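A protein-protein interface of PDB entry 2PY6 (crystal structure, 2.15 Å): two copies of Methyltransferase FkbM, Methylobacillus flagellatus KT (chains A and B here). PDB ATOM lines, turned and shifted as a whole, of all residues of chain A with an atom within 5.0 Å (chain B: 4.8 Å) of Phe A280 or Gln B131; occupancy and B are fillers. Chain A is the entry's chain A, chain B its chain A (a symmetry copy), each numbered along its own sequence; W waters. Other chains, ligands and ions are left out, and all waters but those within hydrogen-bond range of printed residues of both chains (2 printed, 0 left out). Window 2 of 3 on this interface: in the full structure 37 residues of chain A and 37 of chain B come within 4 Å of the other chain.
Ile A245 touches Gln B131.
CG2 of Ile A245 touches NH2 of Arg B134, at 3.5 Å.
Gly A250 touches Gln B131 (CA to OE1, 3.9 Å).
Thr A278 touches Gln B131 (CG2 to NE2, 3.5 Å).
Thr B135 touches Thr A278.
Gln B131 touches Phe A280.
No position is printed for both chains.
Water W2 bridges the side-chain amide oxygen of Asn A279 and the side-chain amide nitrogen of Gln B131.
Water W1 bridges NE2 of Gln B131 (3.3 Å) and O of Gly A250 (3.3 Å).
The backbone NH of Gly A250 sits close to the guanidinium group of Arg B134.
The backbone NH of Gly A250 is in hydrogen-bond range of the backbone carbonyl oxygen of Ile A245 (2.9 Å).
O of Tyr A275 lies within hydrogen-bond range of OG1 of Thr A278 (2.8 Å).
N of Phe A280 lies close to OG1 of Thr A278 (3.4 Å).
The side-chain hydroxyl (OG1) of Thr A278 is in hydrogen-bond range of the backbone NH (N) of Ala A281, 3.2 Å away.
OE1 of Gln B131 sits at hydrogen-bond distance from NH2 of Arg B134 (2.8 Å).
OG1 of Thr B135 sits at hydrogen-bond distance from NE2 of Gln B131, at 2.9 Å.
Gln B131 touches four residues of chain A.
Of the printed residues of chain B, Gly A250 touches Gln B131 (3.9 Å) and Arg B134 (3.5 Å).
Printed residues of chain B within 4 Å of Thr A278: Gln B131 (3.5 Å) and Thr B135 (3.5 Å).
Of the printed residues of chain B, Ile A245 touches Gln B131 and Arg B134.
Of the printed residues of chain A, Arg B134 touches Ile A245 (3.5 Å) and Gly A250 (3.5 Å).
The nearest printed residue of chain B that does not touch Ile A245 is Arg B127 (6.1 Å).
Printed residues of chain B that touch a printed residue of chain A: Gln B131, Arg B134 and Thr B135.
Among the printed residues, 7 pairs touch across the chains.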
ATOM      1  N   ILE A 245      -6.914  -5.873 -32.738  1.00  0.00           N
ATOM      2  CA  ILE A 245      -5.613  -6.472 -32.403  1.00  0.00           C
ATOM      3  C   ILE A 245      -5.605  -7.963 -32.759  1.00  0.00           C
ATOM      4  O   ILE A 245      -4.671  -8.451 -33.407  1.00  0.00           O
ATOM      5  CB  ILE A 245      -5.254  -6.281 -30.906  1.00  0.00           C
ATOM      6  CG1 ILE A 245      -4.982  -4.809 -30.609  1.00  0.00           C
ATOM      7  CG2 ILE A 245      -4.008  -7.120 -30.541  1.00  0.00           C
ATOM      8  CD1 ILE A 245      -4.993  -4.451 -29.119  1.00  0.00           C
ATOM      9  N   GLY A 250      -1.878  -8.052 -34.038  1.00  0.00           N
ATOM     10  CA  GLY A 250      -1.109  -6.937 -33.497  1.00  0.00           C
ATOM     11  C   GLY A 250      -0.491  -6.018 -34.521  1.00  0.00           C
ATOM     12  O   GLY A 250       0.531  -5.448 -34.272  1.00  0.00           O
ATOM     13  N   PHE A 252      -1.440  -2.785 -37.011  1.00  0.00           N
ATOM     14  CA  PHE A 252      -2.283  -1.719 -37.578  1.00  0.00           C
ATOM     15  C   PHE A 252      -1.512  -0.401 -37.589  1.00  0.00           C
ATOM     16  O   PHE A 252      -0.456  -0.300 -36.996  1.00  0.00           O
ATOM     17  CB  PHE A 252      -3.627  -1.595 -36.836  1.00  0.00           C
ATOM     18  CG  PHE A 252      -3.488  -1.418 -35.359  1.00  0.00           C
ATOM     19  CD1 PHE A 252      -3.366  -0.142 -34.814  1.00  0.00           C
ATOM     20  CD2 PHE A 252      -3.458  -2.523 -34.518  1.00  0.00           C
ATOM     21  CE1 PHE A 252      -3.218   0.035 -33.459  1.00  0.00           C
ATOM     22  CE2 PHE A 252      -3.312  -2.360 -33.157  1.00  0.00           C
ATOM     23  CZ  PHE A 252      -3.185  -1.075 -32.629  1.00  0.00           C
ATOM     24  N   TYR A 275      -1.397  -2.685 -22.969  1.00  0.00           N
ATOM     25  CA  TYR A 275      -0.646  -2.677 -24.213  1.00  0.00           C
ATOM     26  C   TYR A 275       0.550  -1.782 -24.210  1.00  0.00           C
ATOM     27  O   TYR A 275       1.182  -1.622 -25.234  1.00  0.00           O
ATOM     28  CB  TYR A 275      -1.568  -2.251 -25.338  1.00  0.00           C
ATOM     29  CG  TYR A 275      -2.773  -3.138 -25.467  1.00  0.00           C
ATOM     30  CD1 TYR A 275      -2.636  -4.486 -25.752  1.00  0.00           C
ATOM     31  CD2 TYR A 275      -4.051  -2.621 -25.353  1.00  0.00           C
ATOM     32  CE1 TYR A 275      -3.757  -5.318 -25.878  1.00  0.00           C
ATOM     33  CE2 TYR A 275      -5.176  -3.430 -25.486  1.00  0.00           C
ATOM     34  CZ  TYR A 275      -5.034  -4.774 -25.752  1.00  0.00           C
ATOM     35  OH  TYR A 275      -6.163  -5.563 -25.891  1.00  0.00           O
ATOM     36  N   THR A 278       3.704  -2.987 -26.053  1.00  0.00           N
ATOM     37  CA  THR A 278       3.548  -3.472 -27.435  1.00  0.00           C
ATOM     38  C   THR A 278       4.180  -2.454 -28.376  1.00  0.00           C
ATOM     39  O   THR A 278       4.435  -1.318 -27.968  1.00  0.00           O
ATOM     40  CB  THR A 278       2.075  -3.646 -27.829  1.00  0.00           C
ATOM     41  OG1 THR A 278       1.428  -2.357 -27.911  1.00  0.00           O
ATOM     42  CG2 THR A 278       1.334  -4.554 -26.838  1.00  0.00           C
ATOM     43  N   ASN A 279       4.450  -2.827 -29.628  1.00  0.00           N
ATOM     44  CA  ASN A 279       5.004  -1.820 -30.570  1.00  0.00           C
ATOM     45  C   ASN A 279       3.929  -0.898 -31.193  1.00  0.00           C
ATOM     46  O   ASN A 279       4.276   0.015 -31.925  1.00  0.00           O
ATOM     47  CB  ASN A 279       5.910  -2.451 -31.644  1.00  0.00           C
ATOM     48  CG  ASN A 279       5.144  -3.325 -32.622  1.00  0.00           C
ATOM     49  OD1 ASN A 279       3.945  -3.576 -32.456  1.00  0.00           O
ATOM     50  ND2 ASN A 279       5.839  -3.805 -33.649  1.00  0.00           N
ATOM     51  N   PHE A 280       2.646  -1.132 -30.881  1.00  0.00           N
ATOM     52  CA  PHE A 280       1.502  -0.339 -31.390  1.00  0.00           C
ATOM     53  C   PHE A 280       0.821   0.597 -30.374  1.00  0.00           C
ATOM     54  O   PHE A 280      -0.142   1.270 -30.715  1.00  0.00           O
ATOM     55  CB  PHE A 280       0.427  -1.248 -32.029  1.00  0.00           C
ATOM     56  CG  PHE A 280      -0.178  -2.290 -31.082  1.00  0.00           C
ATOM     57  CD1 PHE A 280      -1.119  -1.942 -30.116  1.00  0.00           C
ATOM     58  CD2 PHE A 280       0.152  -3.626 -31.207  1.00  0.00           C
ATOM     59  CE1 PHE A 280      -1.685  -2.901 -29.287  1.00  0.00           C
ATOM     60  CE2 PHE A 280      -0.412  -4.586 -30.370  1.00  0.00           C
ATOM     61  CZ  PHE A 280      -1.334  -4.223 -29.425  1.00  0.00           C
ATOM     62  N   ALA A 281       1.315   0.645 -29.143  1.00  0.00           N
ATOM     63  CA  ALA A 281       0.765   1.524 -28.095  1.00  0.00           C
ATOM     64  C   ALA A 281       0.691   3.000 -28.489  1.00  0.00           C
ATOM     65  O   ALA A 281      -0.258   3.714 -28.118  1.00  0.00           O
ATOM     66  CB  ALA A 281       1.597   1.384 -26.835  1.00  0.00           C
ATOM     67  N   SER A 282       1.696   3.457 -29.234  1.00  0.00           N
ATOM     68  CA  SER A 282       1.810   4.861 -29.636  1.00  0.00           C
ATOM     69  C   SER A 282       0.847   5.230 -30.743  1.00  0.00           C
ATOM     70  O   SER A 282       0.637   6.404 -31.000  1.00  0.00           O
ATOM     71  CB  SER A 282       3.245   5.174 -30.090  1.00  0.00           C
ATOM     72  OG  SER A 282       3.673   4.330 -31.168  1.00  0.00           O
ATOM     73  N   ARG A 283       0.258   4.230 -31.384  1.00  0.00           N
ATOM     74  CA  ARG A 283      -0.669   4.436 -32.490  1.00  0.00           C
ATOM     75  C   ARG A 283      -2.121   4.572 -32.045  1.00  0.00           C
ATOM     76  O   ARG A 283      -2.988   4.811 -32.870  1.00  0.00           O
ATOM     77  CB  ARG A 283      -0.558   3.282 -33.478  1.00  0.00           C
ATOM     78  CG  ARG A 283       0.806   3.126 -34.075  1.00  0.00           C
ATOM     79  CD  ARG A 283       0.963   1.768 -34.713  1.00  0.00           C
ATOM     80  NE  ARG A 283       2.332   1.554 -35.175  1.00  0.00           N
ATOM     81  CZ  ARG A 283       2.842   0.387 -35.571  1.00  0.00           C
ATOM     82  NH1 ARG A 283       2.122  -0.741 -35.561  1.00  0.00           N
ATOM     83  NH2 ARG A 283       4.109   0.346 -35.969  1.00  0.00           N
ATOM     84  N   ILE A 284      -2.369   4.451 -30.744  1.00  0.00           N
ATOM     85  CA  ILE A 284      -3.709   4.507 -30.210  1.00  0.00           C
ATOM     86  C   ILE A 284      -3.897   5.770 -29.421  1.00  0.00           C
ATOM     87  O   ILE A 284      -3.085   6.055 -28.551  1.00  0.00           O
ATOM     88  CB  ILE A 284      -3.980   3.320 -29.186  1.00  0.00           C
ATOM     89  CG1 ILE A 284      -3.832   1.945 -29.842  1.00  0.00           C
ATOM     90  CG2 ILE A 284      -5.354   3.410 -28.617  1.00  0.00           C
ATOM     91  CD1 ILE A 284      -3.394   0.857 -28.855  1.00  0.00           C
ATOM     92  N   ARG B 127      -5.901 -14.614 -27.205  1.00  0.00           N
ATOM     93  CA  ARG B 127      -5.397 -13.279 -27.578  1.00  0.00           C
ATOM     94  C   ARG B 127      -4.376 -12.744 -26.576  1.00  0.00           C
ATOM     95  O   ARG B 127      -3.464 -12.045 -26.940  1.00  0.00           O
ATOM     96  CB  ARG B 127      -6.562 -12.268 -27.647  1.00  0.00           C
ATOM     97  CG  ARG B 127      -7.526 -12.496 -28.783  1.00  0.00           C
ATOM     98  CD  ARG B 127      -8.731 -11.575 -28.662  1.00  0.00           C
ATOM     99  NE  ARG B 127      -9.498 -11.649 -29.893  1.00  0.00           N
ATOM    100  CZ  ARG B 127     -10.638 -11.012 -30.122  1.00  0.00           C
ATOM    101  NH1 ARG B 127     -11.215 -10.288 -29.193  1.00  0.00           N
ATOM    102  NH2 ARG B 127     -11.225 -11.159 -31.288  1.00  0.00           N
ATOM    103  N   PHE B 128      -4.583 -13.046 -25.300  1.00  0.00           N
ATOM    104  CA  PHE B 128      -3.646 -12.653 -24.273  1.00  0.00           C
ATOM    105  C   PHE B 128      -2.263 -13.264 -24.578  1.00  0.00           C
ATOM    106  O   PHE B 128      -1.288 -12.567 -24.813  1.00  0.00           O
ATOM    107  CB  PHE B 128      -4.146 -13.089 -22.881  1.00  0.00           C
ATOM    108  CG  PHE B 128      -3.093 -12.972 -21.839  1.00  0.00           C
ATOM    109  CD1 PHE B 128      -2.689 -11.716 -21.400  1.00  0.00           C
ATOM    110  CD2 PHE B 128      -2.434 -14.114 -21.360  1.00  0.00           C
ATOM    111  CE1 PHE B 128      -1.669 -11.599 -20.466  1.00  0.00           C
ATOM    112  CE2 PHE B 128      -1.432 -14.006 -20.441  1.00  0.00           C
ATOM    113  CZ  PHE B 128      -1.035 -12.754 -19.991  1.00  0.00           C
ATOM    114  N   PHE B 129      -2.188 -14.578 -24.614  1.00  0.00           N
ATOM    115  CA  PHE B 129      -0.912 -15.240 -24.894  1.00  0.00           C
ATOM    116  C   PHE B 129      -0.279 -14.939 -26.263  1.00  0.00           C
ATOM    117  O   PHE B 129       0.948 -14.926 -26.394  1.00  0.00           O
ATOM    118  CB  PHE B 129      -1.066 -16.738 -24.723  1.00  0.00           C
ATOM    119  CG  PHE B 129      -1.087 -17.198 -23.293  1.00  0.00           C
ATOM    120  CD1 PHE B 129      -0.043 -16.859 -22.416  1.00  0.00           C
ATOM    121  CD2 PHE B 129      -2.060 -18.056 -22.859  1.00  0.00           C
ATOM    122  CE1 PHE B 129      -0.031 -17.344 -21.114  1.00  0.00           C
ATOM    123  CE2 PHE B 129      -2.058 -18.530 -21.557  1.00  0.00           C
ATOM    124  CZ  PHE B 129      -1.032 -18.167 -20.695  1.00  0.00           C
ATOM    125  N   ASP B 130      -1.107 -14.775 -27.289  1.00  0.00           N
ATOM    126  CA  ASP B 130      -0.609 -14.414 -28.602  1.00  0.00           C
ATOM    127  C   ASP B 130       0.026 -13.052 -28.559  1.00  0.00           C
ATOM    128  O   ASP B 130       1.083 -12.883 -29.118  1.00  0.00           O
ATOM    129  CB  ASP B 130      -1.706 -14.468 -29.683  1.00  0.00           C
ATOM    130  CG  ASP B 130      -1.977 -15.898 -30.174  1.00  0.00           C
ATOM    131  OD1 ASP B 130      -1.108 -16.778 -29.960  1.00  0.00           O
ATOM    132  OD2 ASP B 130      -3.069 -16.144 -30.739  1.00  0.00           O
ATOM    133  N   GLN B 131      -0.587 -12.085 -27.872  1.00  0.00           N
ATOM    134  CA  GLN B 131       0.032 -10.781 -27.781  1.00  0.00           C
ATOM    135  C   GLN B 131       1.268 -10.827 -26.888  1.00  0.00           C
ATOM    136  O   GLN B 131       2.232 -10.198 -27.202  1.00  0.00           O
ATOM    137  CB  GLN B 131      -0.947  -9.688 -27.349  1.00  0.00           C
ATOM    138  CG  GLN B 131      -0.340  -8.284 -27.408  1.00  0.00           C
ATOM    139  CD  GLN B 131       0.251  -7.915 -28.771  1.00  0.00           C
ATOM    140  OE1 GLN B 131      -0.427  -7.992 -29.806  1.00  0.00           O
ATOM    141  NE2 GLN B 131       1.524  -7.496 -28.771  1.00  0.00           N
ATOM    142  N   ILE B 132       1.254 -11.535 -25.766  1.00  0.00           N
ATOM    143  CA  ILE B 132       2.475 -11.658 -24.959  1.00  0.00           C
ATOM    144  C   ILE B 132       3.655 -12.105 -25.819  1.00  0.00           C
ATOM    145  O   ILE B 132       4.756 -11.550 -25.728  1.00  0.00           O
ATOM    146  CB  ILE B 132       2.318 -12.712 -23.822  1.00  0.00           C
ATOM    147  CG1 ILE B 132       1.390 -12.187 -22.718  1.00  0.00           C
ATOM    148  CG2 ILE B 132       3.687 -13.120 -23.242  1.00  0.00           C
ATOM    149  CD1 ILE B 132       1.839 -10.902 -22.072  1.00  0.00           C
ATOM    150  N   CYS B 133       3.418 -13.119 -26.649  1.00  0.00           N
ATOM    151  CA  CYS B 133       4.449 -13.650 -27.521  1.00  0.00           C
ATOM    152  C   CYS B 133       4.901 -12.625 -28.524  1.00  0.00           C
ATOM    153  O   CYS B 133       6.095 -12.448 -28.690  1.00  0.00           O
ATOM    154  CB  CYS B 133       3.976 -14.930 -28.221  1.00  0.00           C
ATOM    155  SG  CYS B 133       3.757 -16.324 -27.055  1.00  0.00           S
ATOM    156  N   ARG B 134       3.961 -11.936 -29.178  1.00  0.00           N
ATOM    157  CA  ARG B 134       4.315 -10.909 -30.183  1.00  0.00           C
ATOM    158  C   ARG B 134       5.115  -9.766 -29.596  1.00  0.00           C
ATOM    159  O   ARG B 134       6.141  -9.369 -30.162  1.00  0.00           O
ATOM    160  CB  ARG B 134       3.079 -10.365 -30.917  1.00  0.00           C
ATOM    161  CG  ARG B 134       2.368 -11.427 -31.782  1.00  0.00           C
ATOM    162  CD  ARG B 134       1.301 -10.810 -32.651  1.00  0.00           C
ATOM    163  NE  ARG B 134       0.187 -10.154 -31.935  1.00  0.00           N
ATOM    164  CZ  ARG B 134      -1.040 -10.661 -31.742  1.00  0.00           C
ATOM    165  NH1 ARG B 134      -1.367 -11.866 -32.168  1.00  0.00           N
ATOM    166  NH2 ARG B 134      -1.973  -9.953 -31.108  1.00  0.00           N
ATOM    167  N   THR B 135       4.658  -9.258 -28.455  1.00  0.00           N
ATOM    168  CA  THR B 135       5.353  -8.187 -27.732  1.00  0.00           C
ATOM    169  C   THR B 135       6.823  -8.549 -27.508  1.00  0.00           C
ATOM    170  O   THR B 135       7.706  -7.734 -27.717  1.00  0.00           O
ATOM    171  CB  THR B 135       4.663  -7.913 -26.341  1.00  0.00           C
ATOM    172  OG1 THR B 135       3.363  -7.336 -26.539  1.00  0.00           O
ATOM    173  CG2 THR B 135       5.468  -6.956 -25.498  1.00  0.00           C
HETATM  174  O   HOH W   1       2.349  -6.935 -31.920  1.00  0.00           O
HETATM  175  O   HOH W   2       3.955  -5.768 -30.389  1.00  0.00           O
